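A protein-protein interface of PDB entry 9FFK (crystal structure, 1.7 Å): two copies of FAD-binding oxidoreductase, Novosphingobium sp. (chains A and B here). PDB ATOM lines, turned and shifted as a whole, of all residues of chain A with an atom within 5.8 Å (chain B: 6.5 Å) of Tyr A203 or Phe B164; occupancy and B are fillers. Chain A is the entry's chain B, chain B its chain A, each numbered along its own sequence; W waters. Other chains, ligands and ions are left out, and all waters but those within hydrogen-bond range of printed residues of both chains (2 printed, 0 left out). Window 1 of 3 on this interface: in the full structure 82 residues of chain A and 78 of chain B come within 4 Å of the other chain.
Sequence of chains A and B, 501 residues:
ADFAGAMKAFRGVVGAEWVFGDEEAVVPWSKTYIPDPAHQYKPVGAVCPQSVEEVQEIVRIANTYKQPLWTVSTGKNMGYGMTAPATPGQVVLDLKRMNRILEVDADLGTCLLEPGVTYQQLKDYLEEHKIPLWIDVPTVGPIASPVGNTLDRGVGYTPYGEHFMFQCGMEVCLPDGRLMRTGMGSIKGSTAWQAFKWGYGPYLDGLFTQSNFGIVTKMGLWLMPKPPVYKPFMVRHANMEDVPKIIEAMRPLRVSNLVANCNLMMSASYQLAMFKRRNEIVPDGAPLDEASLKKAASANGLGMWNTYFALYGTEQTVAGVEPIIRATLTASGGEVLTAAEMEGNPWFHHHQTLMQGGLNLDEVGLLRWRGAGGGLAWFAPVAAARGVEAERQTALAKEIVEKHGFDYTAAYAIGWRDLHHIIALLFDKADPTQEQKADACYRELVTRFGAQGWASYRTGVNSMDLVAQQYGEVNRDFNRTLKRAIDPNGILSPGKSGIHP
Printed residues of chain A that touch a printed residue of chain B: Phe A164, Met A165, Trp A198, Gly A199, Gly A201, Pro A202, Tyr A203, Leu A204, Gly A206 and Leu A207. Hydrophobic or aromatic side chains of chain A within 4 Å of the printed part of chain B: Phe A164, Met A165, Trp A198, Pro A202, Tyr A203, Leu A204 and Leu A207. Hydrophobic or aromatic side chains of chain B that line the printed part of chain A: Phe B164, Met B165, Tyr B203, Leu B204 and Leu B207.
Of the printed residues of chain B, Pro A202 touches Gly B206, Leu B207, Thr B209, Gln B210 and Ser B211. Printed residues of chain B within 4 Å of Leu A207: Tyr B203 (3.6 Å), Leu B204 (3.8 Å) and Leu B207 (3.6 Å). Phe B164 touches just these residues of chain A: Trp A198 (3.6 Å) and Tyr A203 (3.7 Å). The nearest residue of chain A that does not touch Phe B164 is Met A165 (5.5 Å). The nearest printed residue of chain B that does not touch Leu A204 is Gly B206 (5.4 Å).
O of Gly A199 lies within hydrogen-bond range of NH2 of Arg B153 (3.2 Å). The backbone carbonyl oxygen (O) of Gly A201 sits at hydrogen-bond distance from the guanidinium group (NH2) of Arg B153 (2.8 Å). NE1 of Trp A198 sits at hydrogen-bond distance from OE2 of Glu B162 (2.7 Å). The backbone carbonyl oxygen (O) of Gly A206 is in hydrogen-bond range of the backbone NH (N) of Tyr B203. O of Gly B206 is in hydrogen-bond range of N of Tyr A203 (3.0 Å). OE1 of Gln B210 sits at hydrogen-bond distance from N of Gly A201 (3.0 Å). N of Pro A202 lies close to O of Gln B210, 3.4 Å away.
Water W2 lies within hydrogen-bond range of O of Gly A199 (2.7 Å), NE of Arg B153 (2.9 Å) and NE2 of Gln B210 (3.5 Å).
O of Gly B206 is in hydrogen-bond range of OG1 of Thr B209, 2.7 Å away. O of Phe A164 sits at hydrogen-bond distance from NZ of Lys A197, at 3.4 Å. NZ of Lys A197 lies within hydrogen-bond range of O of Met A165, at 2.9 Å.
Phe A164 touches Tyr B203, and with the chains exchanged Tyr A203 touches Phe B164. Met B165 touches its own counterpart, Met A165. Leu A207 touches its own counterpart, Leu B207. 9 positions are printed for both chains.
Phe A164 touches Tyr B203. CZ3 of Trp A198 touches CD2 of Phe B164, at 3.6 Å. Gly A201 touches Thr B209. Tyr A203 touches Arg B153. Phe B164 touches Tyr A203 (CE2 to CD2, 3.7 Å). N of Leu A207 touches O of Tyr B203, 3.6 Å away. Leu A207 touches Leu B204.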
ATOM      1  N   PHE A 164      13.415  -8.774 -11.229  1.00  0.00           N
ATOM      2  CA  PHE A 164      14.842  -8.991 -11.516  1.00  0.00           C
ATOM      3  C   PHE A 164      15.451 -10.058 -10.576  1.00  0.00           C
ATOM      4  O   PHE A 164      16.340 -10.761 -11.027  1.00  0.00           O
ATOM      5  CB  PHE A 164      15.579  -7.665 -11.516  1.00  0.00           C
ATOM      6  CG  PHE A 164      17.032  -7.806 -11.886  1.00  0.00           C
ATOM      7  CD1 PHE A 164      17.434  -8.540 -12.998  1.00  0.00           C
ATOM      8  CD2 PHE A 164      18.000  -7.147 -11.148  1.00  0.00           C
ATOM      9  CE1 PHE A 164      18.790  -8.640 -13.331  1.00  0.00           C
ATOM     10  CE2 PHE A 164      19.348  -7.262 -11.477  1.00  0.00           C
ATOM     11  CZ  PHE A 164      19.728  -7.999 -12.577  1.00  0.00           C
ATOM     12  N   MET A 165      14.995 -10.247  -9.326  1.00  0.00           N
ATOM     13  CA  MET A 165      15.576 -11.297  -8.443  1.00  0.00           C
ATOM     14  C   MET A 165      15.331 -12.717  -9.032  1.00  0.00           C
ATOM     15  O   MET A 165      16.172 -13.648  -8.797  1.00  0.00           O
ATOM     16  CB  MET A 165      15.073 -11.183  -7.000  1.00  0.00           C
ATOM     17  CG  MET A 165      15.725 -12.200  -6.037  1.00  0.00           C
ATOM     18  SD  MET A 165      17.555 -12.329  -6.125  1.00  0.00           S
ATOM     19  CE  MET A 165      18.225 -11.511  -4.683  1.00  0.00           C
ATOM     20  N   GLN A 167      15.018 -13.420 -12.396  1.00  0.00           N
ATOM     21  CA  GLN A 167      15.594 -13.610 -13.742  1.00  0.00           C
ATOM     22  C   GLN A 167      16.806 -14.540 -13.623  1.00  0.00           C
ATOM     23  O   GLN A 167      17.574 -14.427 -12.665  1.00  0.00           O
ATOM     24  CB  GLN A 167      15.972 -12.210 -14.286  1.00  0.00           C
ATOM     25  CG  GLN A 167      16.588 -12.240 -15.674  1.00  0.00           C
ATOM     26  CD  GLN A 167      18.100 -12.212 -15.707  1.00  0.00           C
ATOM     27  OE1 GLN A 167      18.749 -12.835 -16.568  1.00  0.00           O
ATOM     28  NE2 GLN A 167      18.668 -11.686 -14.672  1.00  0.00           N
ATOM     29  N   LYS A 197      22.018 -18.442 -11.307  1.00  0.00           N
ATOM     30  CA  LYS A 197      22.038 -17.046 -11.817  1.00  0.00           C
ATOM     31  C   LYS A 197      23.462 -16.588 -12.158  1.00  0.00           C
ATOM     32  O   LYS A 197      23.597 -15.873 -13.180  1.00  0.00           O
ATOM     33  CB  LYS A 197      21.432 -15.998 -10.877  1.00  0.00           C
ATOM     34  CG  LYS A 197      19.983 -16.194 -10.439  1.00  0.00           C
ATOM     35  CD  LYS A 197      19.533 -15.229  -9.340  1.00  0.00           C
ATOM     36  CE  LYS A 197      19.782 -13.756  -9.618  1.00  0.00           C
ATOM     37  NZ  LYS A 197      18.597 -13.167 -10.289  1.00  0.00           N
ATOM     38  N   TRP A 198      24.481 -16.862 -11.330  1.00  0.00           N
ATOM     39  CA  TRP A 198      25.659 -15.931 -11.298  1.00  0.00           C
ATOM     40  C   TRP A 198      26.667 -16.254 -12.412  1.00  0.00           C
ATOM     41  O   TRP A 198      27.430 -15.338 -12.838  1.00  0.00           O
ATOM     42  CB  TRP A 198      26.379 -15.982  -9.947  1.00  0.00           C
ATOM     43  CG  TRP A 198      25.549 -15.902  -8.702  1.00  0.00           C
ATOM     44  CD1 TRP A 198      25.594 -16.758  -7.638  1.00  0.00           C
ATOM     45  CD2 TRP A 198      24.524 -14.951  -8.413  1.00  0.00           C
ATOM     46  NE1 TRP A 198      24.748 -16.340  -6.661  1.00  0.00           N
ATOM     47  CE2 TRP A 198      24.091 -15.210  -7.099  1.00  0.00           C
ATOM     48  CE3 TRP A 198      24.006 -13.850  -9.111  1.00  0.00           C
ATOM     49  CZ2 TRP A 198      23.028 -14.507  -6.535  1.00  0.00           C
ATOM     50  CZ3 TRP A 198      23.023 -13.086  -8.517  1.00  0.00           C
ATOM     51  CH2 TRP A 198      22.525 -13.435  -7.248  1.00  0.00           C
ATOM     52  N   GLY A 199      26.750 -17.531 -12.794  1.00  0.00           N
ATOM     53  CA  GLY A 199      27.902 -18.046 -13.551  1.00  0.00           C
ATOM     54  C   GLY A 199      29.232 -17.820 -12.862  1.00  0.00           C
ATOM     55  O   GLY A 199      29.341 -18.061 -11.677  1.00  0.00           O
ATOM     56  N   GLY A 201      32.977 -15.454 -12.719  1.00  0.00           N
ATOM     57  CA  GLY A 201      33.605 -14.160 -13.038  1.00  0.00           C
ATOM     58  C   GLY A 201      32.551 -13.089 -12.827  1.00  0.00           C
ATOM     59  O   GLY A 201      31.494 -13.358 -12.220  1.00  0.00           O
ATOM     60  N   PRO A 202      32.787 -11.857 -13.313  1.00  0.00           N
ATOM     61  CA  PRO A 202      31.856 -10.759 -13.054  1.00  0.00           C
ATOM     62  C   PRO A 202      30.425 -11.133 -13.486  1.00  0.00           C
ATOM     63  O   PRO A 202      30.221 -11.708 -14.537  1.00  0.00           O
ATOM     64  CB  PRO A 202      32.433  -9.543 -13.817  1.00  0.00           C
ATOM     65  CG  PRO A 202      33.690 -10.024 -14.481  1.00  0.00           C
ATOM     66  CD  PRO A 202      33.955 -11.471 -14.121  1.00  0.00           C
ATOM     67  N   TYR A 203      29.446 -10.842 -12.622  1.00  0.00           N
ATOM     68  CA  TYR A 203      28.011 -11.043 -12.883  1.00  0.00           C
ATOM     69  C   TYR A 203      27.461  -9.860 -13.686  1.00  0.00           C
ATOM     70  O   TYR A 203      27.411  -8.723 -13.136  1.00  0.00           O
ATOM     71  CB  TYR A 203      27.248 -11.198 -11.576  1.00  0.00           C
ATOM     72  CG  TYR A 203      25.765 -11.142 -11.720  1.00  0.00           C
ATOM     73  CD1 TYR A 203      25.089 -12.082 -12.446  1.00  0.00           C
ATOM     74  CD2 TYR A 203      25.021 -10.177 -11.075  1.00  0.00           C
ATOM     75  CE1 TYR A 203      23.718 -12.090 -12.547  1.00  0.00           C
ATOM     76  CE2 TYR A 203      23.631 -10.180 -11.144  1.00  0.00           C
ATOM     77  CZ  TYR A 203      22.971 -11.157 -11.866  1.00  0.00           C
ATOM     78  OH  TYR A 203      21.603 -11.197 -11.961  1.00  0.00           O
ATOM     79  N   LEU A 204      27.047 -10.142 -14.921  1.00  0.00           N
ATOM     80  CA  LEU A 204      26.846  -9.033 -15.888  1.00  0.00           C
ATOM     81  C   LEU A 204      25.380  -8.758 -16.176  1.00  0.00           C
ATOM     82  O   LEU A 204      25.121  -7.767 -16.875  1.00  0.00           O
ATOM     83  CB  LEU A 204      27.631  -9.369 -17.151  1.00  0.00           C
ATOM     84  CG  LEU A 204      29.156  -9.414 -16.991  1.00  0.00           C
ATOM     85  CD1 LEU A 204      29.795  -9.460 -18.353  1.00  0.00           C
ATOM     86  CD2 LEU A 204      29.694  -8.212 -16.224  1.00  0.00           C
ATOM     87  N   ASP A 205      24.432  -9.564 -15.697  1.00  0.00           N
ATOM     88  CA  ASP A 205      23.062  -9.449 -16.173  1.00  0.00           C
ATOM     89  C   ASP A 205      22.540  -8.089 -15.787  1.00  0.00           C
ATOM     90  O   ASP A 205      21.736  -7.515 -16.596  1.00  0.00           O
ATOM     91  CB  ASP A 205      22.168 -10.605 -15.660  1.00  0.00           C
ATOM     92  CG  ASP A 205      22.613 -12.003 -16.043  1.00  0.00           C
ATOM     93  OD1 ASP A 205      23.719 -12.381 -15.677  1.00  0.00           O
ATOM     94  OD2 ASP A 205      21.858 -12.704 -16.639  1.00  0.00           O
ATOM     95  N   GLY A 206      22.876  -7.585 -14.597  1.00  0.00           N
ATOM     96  CA  GLY A 206      22.475  -6.229 -14.172  1.00  0.00           C
ATOM     97  C   GLY A 206      22.854  -5.109 -15.129  1.00  0.00           C
ATOM     98  O   GLY A 206      22.141  -4.018 -15.183  1.00  0.00           O
ATOM     99  N   LEU A 207      23.980  -5.280 -15.821  1.00  0.00           N
ATOM    100  CA  LEU A 207      24.420  -4.286 -16.825  1.00  0.00           C
ATOM    101  C   LEU A 207      23.367  -4.053 -17.911  1.00  0.00           C
ATOM    102  O   LEU A 207      23.477  -2.998 -18.583  1.00  0.00           O
ATOM    103  CB  LEU A 207      25.697  -4.757 -17.527  1.00  0.00           C
ATOM    104  CG  LEU A 207      26.990  -4.177 -17.014  1.00  0.00           C
ATOM    105  CD1 LEU A 207      27.143  -4.482 -15.541  1.00  0.00           C
ATOM    106  CD2 LEU A 207      28.119  -4.789 -17.802  1.00  0.00           C
ATOM    107  N   THR B 150      31.202 -13.062   0.295  1.00  0.00           N
ATOM    108  CA  THR B 150      30.093 -12.550  -0.557  1.00  0.00           C
ATOM    109  C   THR B 150      30.676 -12.125  -1.926  1.00  0.00           C
ATOM    110  O   THR B 150      30.020 -12.388  -2.975  1.00  0.00           O
ATOM    111  CB  THR B 150      29.253 -11.492   0.169  1.00  0.00           C
ATOM    112  OG1 THR B 150      28.669 -11.980   1.408  1.00  0.00           O
ATOM    113  CG2 THR B 150      28.217 -10.978  -0.789  1.00  0.00           C
ATOM    114  N   LEU B 151      31.853 -11.520  -1.953  1.00  0.00           N
ATOM    115  CA  LEU B 151      32.424 -11.036  -3.245  1.00  0.00           C
ATOM    116  C   LEU B 151      32.883 -12.206  -4.147  1.00  0.00           C
ATOM    117  O   LEU B 151      32.908 -12.029  -5.424  1.00  0.00           O
ATOM    118  CB  LEU B 151      33.517  -9.999  -3.021  1.00  0.00           C
ATOM    119  CG  LEU B 151      33.051  -8.739  -2.281  1.00  0.00           C
ATOM    120  CD1 LEU B 151      34.243  -7.908  -1.886  1.00  0.00           C
ATOM    121  CD2 LEU B 151      32.063  -7.937  -3.078  1.00  0.00           C
ATOM    122  N   ARG B 153      31.046 -14.906  -4.082  1.00  0.00           N
ATOM    123  CA  ARG B 153      29.674 -15.475  -4.173  1.00  0.00           C
ATOM    124  C   ARG B 153      29.639 -16.835  -3.497  1.00  0.00           C
ATOM    125  O   ARG B 153      29.158 -17.813  -4.104  1.00  0.00           O
ATOM    126  CB  ARG B 153      29.233 -15.562  -5.635  1.00  0.00           C
ATOM    127  CG  ARG B 153      29.254 -14.201  -6.282  1.00  0.00           C
ATOM    128  CD  ARG B 153      28.543 -14.170  -7.587  1.00  0.00           C
ATOM    129  NE  ARG B 153      29.213 -14.950  -8.625  1.00  0.00           N
ATOM    130  CZ  ARG B 153      29.899 -14.460  -9.627  1.00  0.00           C
ATOM    131  NH1 ARG B 153      30.048 -13.172  -9.752  1.00  0.00           N
ATOM    132  NH2 ARG B 153      30.375 -15.261 -10.565  1.00  0.00           N
ATOM    133  N   GLY B 154      30.148 -16.878  -2.268  1.00  0.00           N
ATOM    134  CA  GLY B 154      30.080 -18.069  -1.429  1.00  0.00           C
ATOM    135  C   GLY B 154      28.717 -18.263  -0.824  1.00  0.00           C
ATOM    136  O   GLY B 154      27.798 -17.430  -1.007  1.00  0.00           O
ATOM    137  N   GLY B 161      21.493 -18.307   2.885  1.00  0.00           N
ATOM    138  CA  GLY B 161      22.700 -18.948   2.388  1.00  0.00           C
ATOM    139  C   GLY B 161      23.360 -18.453   1.123  1.00  0.00           C
ATOM    140  O   GLY B 161      24.544 -18.526   1.010  1.00  0.00           O
ATOM    141  N   GLU B 162      22.577 -17.957   0.187  1.00  0.00           N
ATOM    142  CA  GLU B 162      23.122 -17.425  -1.055  1.00  0.00           C
ATOM    143  C   GLU B 162      23.542 -16.001  -0.804  1.00  0.00           C
ATOM    144  O   GLU B 162      22.817 -15.088  -1.059  1.00  0.00           O
ATOM    145  CB  GLU B 162      22.141 -17.574  -2.207  1.00  0.00           C
ATOM    146  CG  GLU B 162      22.708 -17.300  -3.577  1.00  0.00           C
ATOM    147  CD  GLU B 162      23.755 -18.294  -3.988  1.00  0.00           C
ATOM    148  OE1 GLU B 162      23.513 -19.509  -3.886  1.00  0.00           O
ATOM    149  OE2 GLU B 162      24.821 -17.850  -4.398  1.00  0.00           O
ATOM    150  N   HIS B 163      24.764 -15.849  -0.321  1.00  0.00           N
ATOM    151  CA  HIS B 163      25.227 -14.545   0.109  1.00  0.00           C
ATOM    152  C   HIS B 163      25.047 -13.326  -0.794  1.00  0.00           C
ATOM    153  O   HIS B 163      24.589 -12.311  -0.343  1.00  0.00           O
ATOM    154  CB  HIS B 163      26.652 -14.676   0.620  1.00  0.00           C
ATOM    155  CG  HIS B 163      26.769 -15.560   1.811  1.00  0.00           C
ATOM    156  ND1 HIS B 163      27.946 -16.157   2.175  1.00  0.00           N
ATOM    157  CD2 HIS B 163      25.856 -15.946   2.727  1.00  0.00           C
ATOM    158  CE1 HIS B 163      27.764 -16.877   3.260  1.00  0.00           C
ATOM    159  NE2 HIS B 163      26.504 -16.760   3.619  1.00  0.00           N
ATOM    160  N   PHE B 164      25.397 -13.451  -2.055  1.00  0.00           N
ATOM    161  CA  PHE B 164      25.250 -12.330  -2.942  1.00  0.00           C
ATOM    162  C   PHE B 164      23.771 -11.893  -3.099  1.00  0.00           C
ATOM    163  O   PHE B 164      23.515 -10.731  -3.269  1.00  0.00           O
ATOM    164  CB  PHE B 164      25.969 -12.581  -4.275  1.00  0.00           C
ATOM    165  CG  PHE B 164      25.953 -11.426  -5.222  1.00  0.00           C
ATOM    166  CD1 PHE B 164      26.275 -10.153  -4.809  1.00  0.00           C
ATOM    167  CD2 PHE B 164      25.645 -11.623  -6.550  1.00  0.00           C
ATOM    168  CE1 PHE B 164      26.250  -9.100  -5.700  1.00  0.00           C
ATOM    169  CE2 PHE B 164      25.623 -10.575  -7.446  1.00  0.00           C
ATOM    170  CZ  PHE B 164      25.928  -9.313  -7.017  1.00  0.00           C
ATOM    171  N   MET B 165      22.818 -12.815  -2.963  1.00  0.00           N
ATOM    172  CA  MET B 165      21.393 -12.391  -3.053  1.00  0.00           C
ATOM    173  C   MET B 165      21.083 -11.403  -1.908  1.00  0.00           C
ATOM    174  O   MET B 165      20.218 -10.566  -2.095  1.00  0.00           O
ATOM    175  CB  MET B 165      20.407 -13.558  -2.947  1.00  0.00           C
ATOM    176  CG  MET B 165      20.165 -14.355  -4.200  1.00  0.00           C
ATOM    177  SD  MET B 165      19.007 -15.748  -3.877  1.00  0.00           S
ATOM    178  CE  MET B 165      19.193 -16.783  -5.338  1.00  0.00           C
ATOM    179  N   PHE B 166      21.764 -11.476  -0.776  1.00  0.00           N
ATOM    180  CA  PHE B 166      21.457 -10.696   0.433  1.00  0.00           C
ATOM    181  C   PHE B 166      22.381  -9.490   0.572  1.00  0.00           C
ATOM    182  O   PHE B 166      22.326  -8.833   1.595  1.00  0.00           O
ATOM    183  CB  PHE B 166      21.470 -11.647   1.634  1.00  0.00           C
ATOM    184  CG  PHE B 166      20.383 -12.680   1.497  1.00  0.00           C
ATOM    185  CD1 PHE B 166      19.100 -12.388   1.894  1.00  0.00           C
ATOM    186  CD2 PHE B 166      20.628 -13.906   0.901  1.00  0.00           C
ATOM    187  CE1 PHE B 166      18.073 -13.299   1.706  1.00  0.00           C
ATOM    188  CE2 PHE B 166      19.593 -14.801   0.695  1.00  0.00           C
ATOM    189  CZ  PHE B 166      18.323 -14.496   1.100  1.00  0.00           C
ATOM    190  N   GLN B 167      23.267  -9.235  -0.399  1.00  0.00           N
ATOM    191  CA  GLN B 167      24.139  -8.057  -0.363  1.00  0.00           C
ATOM    192  C   GLN B 167      23.268  -6.879  -0.765  1.00  0.00           C
ATOM    193  O   GLN B 167      22.448  -7.040  -1.648  1.00  0.00           O
ATOM    194  CB  GLN B 167      25.306  -8.293  -1.361  1.00  0.00           C
ATOM    195  CG  GLN B 167      26.269  -7.144  -1.471  1.00  0.00           C
ATOM    196  CD  GLN B 167      25.970  -6.307  -2.694  1.00  0.00           C
ATOM    197  OE1 GLN B 167      25.422  -6.785  -3.667  1.00  0.00           O
ATOM    198  NE2 GLN B 167      26.189  -5.032  -2.589  1.00  0.00           N
ATOM    199  N   CYS B 168      23.468  -5.721  -0.195  1.00  0.00           N
ATOM    200  CA  CYS B 168      22.645  -4.523  -0.501  1.00  0.00           C
ATOM    201  C   CYS B 168      23.478  -3.280  -0.279  1.00  0.00           C
ATOM    202  O   CYS B 168      23.698  -2.910   0.878  1.00  0.00           O
ATOM    203  CB  CYS B 168      21.379  -4.496   0.328  1.00  0.00           C
ATOM    204  SG  CYS B 168      20.212  -3.282  -0.338  1.00  0.00           S
ATOM    205  N   MET B 170      27.185  -1.275  -1.956  1.00  0.00           N
ATOM    206  CA  MET B 170      28.612  -1.422  -1.664  1.00  0.00           C
ATOM    207  C   MET B 170      29.304  -0.063  -2.006  1.00  0.00           C
ATOM    208  O   MET B 170      28.765   0.807  -2.750  1.00  0.00           O
ATOM    209  CB  MET B 170      29.198  -2.604  -2.426  1.00  0.00           C
ATOM    210  CG  MET B 170      29.241  -2.439  -3.920  1.00  0.00           C
ATOM    211  SD  MET B 170      30.142  -3.732  -4.709  1.00  0.00           S
ATOM    212  CE  MET B 170      29.370  -5.270  -4.270  1.00  0.00           C
ATOM    213  N   LYS B 197      18.208  -2.837  -3.299  1.00  0.00           N
ATOM    214  CA  LYS B 197      19.458  -3.307  -3.954  1.00  0.00           C
ATOM    215  C   LYS B 197      19.758  -2.498  -5.217  1.00  0.00           C
ATOM    216  O   LYS B 197      20.923  -2.221  -5.428  1.00  0.00           O
ATOM    217  CB  LYS B 197      19.438  -4.783  -4.322  1.00  0.00           C
ATOM    218  CG  LYS B 197      19.384  -5.811  -3.205  1.00  0.00           C
ATOM    219  CD  LYS B 197      19.073  -7.210  -3.684  1.00  0.00           C
ATOM    220  CE  LYS B 197      20.135  -7.770  -4.599  1.00  0.00           C
ATOM    221  NZ  LYS B 197      21.232  -8.397  -3.801  1.00  0.00           N
ATOM    222  N   TYR B 203      22.606  -2.000 -13.059  1.00  0.00           N
ATOM    223  CA  TYR B 203      22.934  -2.539 -11.730  1.00  0.00           C
ATOM    224  C   TYR B 203      24.366  -3.074 -11.774  1.00  0.00           C
ATOM    225  O   TYR B 203      24.658  -4.064 -12.516  1.00  0.00           O
ATOM    226  CB  TYR B 203      21.853  -3.527 -11.343  1.00  0.00           C
ATOM    227  CG  TYR B 203      22.257  -4.404 -10.192  1.00  0.00           C
ATOM    228  CD1 TYR B 203      22.332  -3.875  -8.924  1.00  0.00           C
ATOM    229  CD2 TYR B 203      22.480  -5.758 -10.345  1.00  0.00           C
ATOM    230  CE1 TYR B 203      22.685  -4.656  -7.831  1.00  0.00           C
ATOM    231  CE2 TYR B 203      22.735  -6.582  -9.242  1.00  0.00           C
ATOM    232  CZ  TYR B 203      22.815  -6.022  -7.985  1.00  0.00           C
ATOM    233  OH  TYR B 203      23.143  -6.780  -6.920  1.00  0.00           O
ATOM    234  N   LEU B 204      25.218  -2.499 -10.965  1.00  0.00           N
ATOM    235  CA  LEU B 204      26.675  -2.734 -11.175  1.00  0.00           C
ATOM    236  C   LEU B 204      27.318  -3.568 -10.083  1.00  0.00           C
ATOM    237  O   LEU B 204      28.499  -3.907 -10.270  1.00  0.00           O
ATOM    238  CB  LEU B 204      27.363  -1.379 -11.284  1.00  0.00           C
ATOM    239  CG  LEU B 204      26.845  -0.468 -12.401  1.00  0.00           C
ATOM    240  CD1 LEU B 204      27.663   0.794 -12.432  1.00  0.00           C
ATOM    241  CD2 LEU B 204      26.850  -1.168 -13.770  1.00  0.00           C
ATOM    242  N   ASP B 205      26.625  -3.885  -8.988  1.00  0.00           N
ATOM    243  CA  ASP B 205      27.259  -4.547  -7.823  1.00  0.00           C
ATOM    244  C   ASP B 205      27.927  -5.830  -8.343  1.00  0.00           C
ATOM    245  O   ASP B 205      28.981  -6.196  -7.819  1.00  0.00           O
ATOM    246  CB  ASP B 205      26.239  -4.736  -6.677  1.00  0.00           C
ATOM    247  CG  ASP B 205      25.633  -3.451  -6.128  1.00  0.00           C
ATOM    248  OD1 ASP B 205      25.062  -2.718  -6.951  1.00  0.00           O
ATOM    249  OD2 ASP B 205      25.769  -3.197  -4.920  1.00  0.00           O
ATOM    250  N   GLY B 206      27.284  -6.560  -9.256  1.00  0.00           N
ATOM    251  CA  GLY B 206      27.784  -7.841  -9.785  1.00  0.00           C
ATOM    252  C   GLY B 206      29.128  -7.712 -10.480  1.00  0.00           C
ATOM    253  O   GLY B 206      29.903  -8.715 -10.529  1.00  0.00           O
ATOM    254  N   LEU B 207      29.373  -6.553 -11.072  1.00  0.00           N
ATOM    255  CA  LEU B 207      30.678  -6.284 -11.713  1.00  0.00           C
ATOM    256  C   LEU B 207      31.845  -6.428 -10.739  1.00  0.00           C
ATOM    257  O   LEU B 207      32.958  -6.573 -11.250  1.00  0.00           O
ATOM    258  CB  LEU B 207      30.741  -4.858 -12.257  1.00  0.00           C
ATOM    259  CG  LEU B 207      30.201  -4.623 -13.650  1.00  0.00           C
ATOM    260  CD1 LEU B 207      30.473  -3.197 -14.036  1.00  0.00           C
ATOM    261  CD2 LEU B 207      30.810  -5.552 -14.665  1.00  0.00           C
ATOM    262  N   PHE B 208      31.609  -6.249  -9.423  1.00  0.00           N
ATOM    263  CA  PHE B 208      32.623  -6.228  -8.349  1.00  0.00           C
ATOM    264  C   PHE B 208      32.627  -7.563  -7.595  1.00  0.00           C
ATOM    265  O   PHE B 208      33.169  -7.610  -6.503  1.00  0.00           O
ATOM    266  CB  PHE B 208      32.397  -4.997  -7.473  1.00  0.00           C
ATOM    267  CG  PHE B 208      32.446  -3.739  -8.304  1.00  0.00           C
ATOM    268  CD1 PHE B 208      33.625  -3.343  -8.867  1.00  0.00           C
ATOM    269  CD2 PHE B 208      31.304  -2.995  -8.567  1.00  0.00           C
ATOM    270  CE1 PHE B 208      33.672  -2.234  -9.696  1.00  0.00           C
ATOM    271  CE2 PHE B 208      31.351  -1.856  -9.363  1.00  0.00           C
ATOM    272  CZ  PHE B 208      32.545  -1.510  -9.966  1.00  0.00           C
ATOM    273  N   THR B 209      32.053  -8.616  -8.197  1.00  0.00           N
ATOM    274  CA  THR B 209      32.038  -9.953  -7.642  1.00  0.00           C
ATOM    275  C   THR B 209      32.779 -10.846  -8.621  1.00  0.00           C
ATOM    276  O   THR B 209      32.701 -10.636  -9.874  1.00  0.00           O
ATOM    277  CB  THR B 209      30.618 -10.465  -7.340  1.00  0.00           C
ATOM    278  OG1 THR B 209      29.872 -10.557  -8.540  1.00  0.00           O
ATOM    279  CG2 THR B 209      29.877  -9.581  -6.392  1.00  0.00           C
ATOM    280  N   GLN B 210      33.630 -11.690  -8.022  1.00  0.00           N
ATOM    281  CA  GLN B 210      34.553 -12.539  -8.746  1.00  0.00           C
ATOM    282  C   GLN B 210      35.228 -11.733  -9.845  1.00  0.00           C
ATOM    283  O   GLN B 210      35.285 -12.189 -11.010  1.00  0.00           O
ATOM    284  CB  GLN B 210      33.872 -13.757  -9.368  1.00  0.00           C
ATOM    285  CG  GLN B 210      33.439 -14.753  -8.295  1.00  0.00           C
ATOM    286  CD  GLN B 210      33.150 -16.151  -8.793  1.00  0.00           C
ATOM    287  OE1 GLN B 210      33.381 -16.493  -9.928  1.00  0.00           O
ATOM    288  NE2 GLN B 210      32.472 -16.965  -7.970  1.00  0.00           N
ATOM    289  N   SER B 211      35.750 -10.582  -9.498  1.00  0.00           N
ATOM    290  CA  SER B 211      36.334  -9.740 -10.563  1.00  0.00           C
ATOM    291  C   SER B 211      37.471  -8.858 -10.091  1.00  0.00           C
ATOM    292  O   SER B 211      37.917  -8.943  -8.937  1.00  0.00           O
ATOM    293  CB  SER B 211      35.267  -8.925 -11.186  1.00  0.00           C
ATOM    294  OG  SER B 211      34.969  -7.892 -10.316  1.00  0.00           O
ATOM    295  N   LEU B 221      24.670  -5.734   3.974  1.00  0.00           N
ATOM    296  CA  LEU B 221      24.201  -7.125   4.009  1.00  0.00           C
ATOM    297  C   LEU B 221      22.896  -7.128   4.763  1.00  0.00           C
ATOM    298  O   LEU B 221      22.814  -6.532   5.852  1.00  0.00           O
ATOM    299  CB  LEU B 221      25.198  -8.009   4.763  1.00  0.00           C
ATOM    300  CG  LEU B 221      25.949  -8.987   3.876  1.00  0.00           C
ATOM    301  CD1 LEU B 221      27.081  -9.619   4.690  1.00  0.00           C
ATOM    302  CD2 LEU B 221      24.987 -10.076   3.312  1.00  0.00           C
HETATM  303  O   HOH W   1      25.532  -6.574 -12.020  1.00  0.00           O
HETATM  304  O   HOH W   2      29.245 -17.802  -8.947  1.00  0.00           O
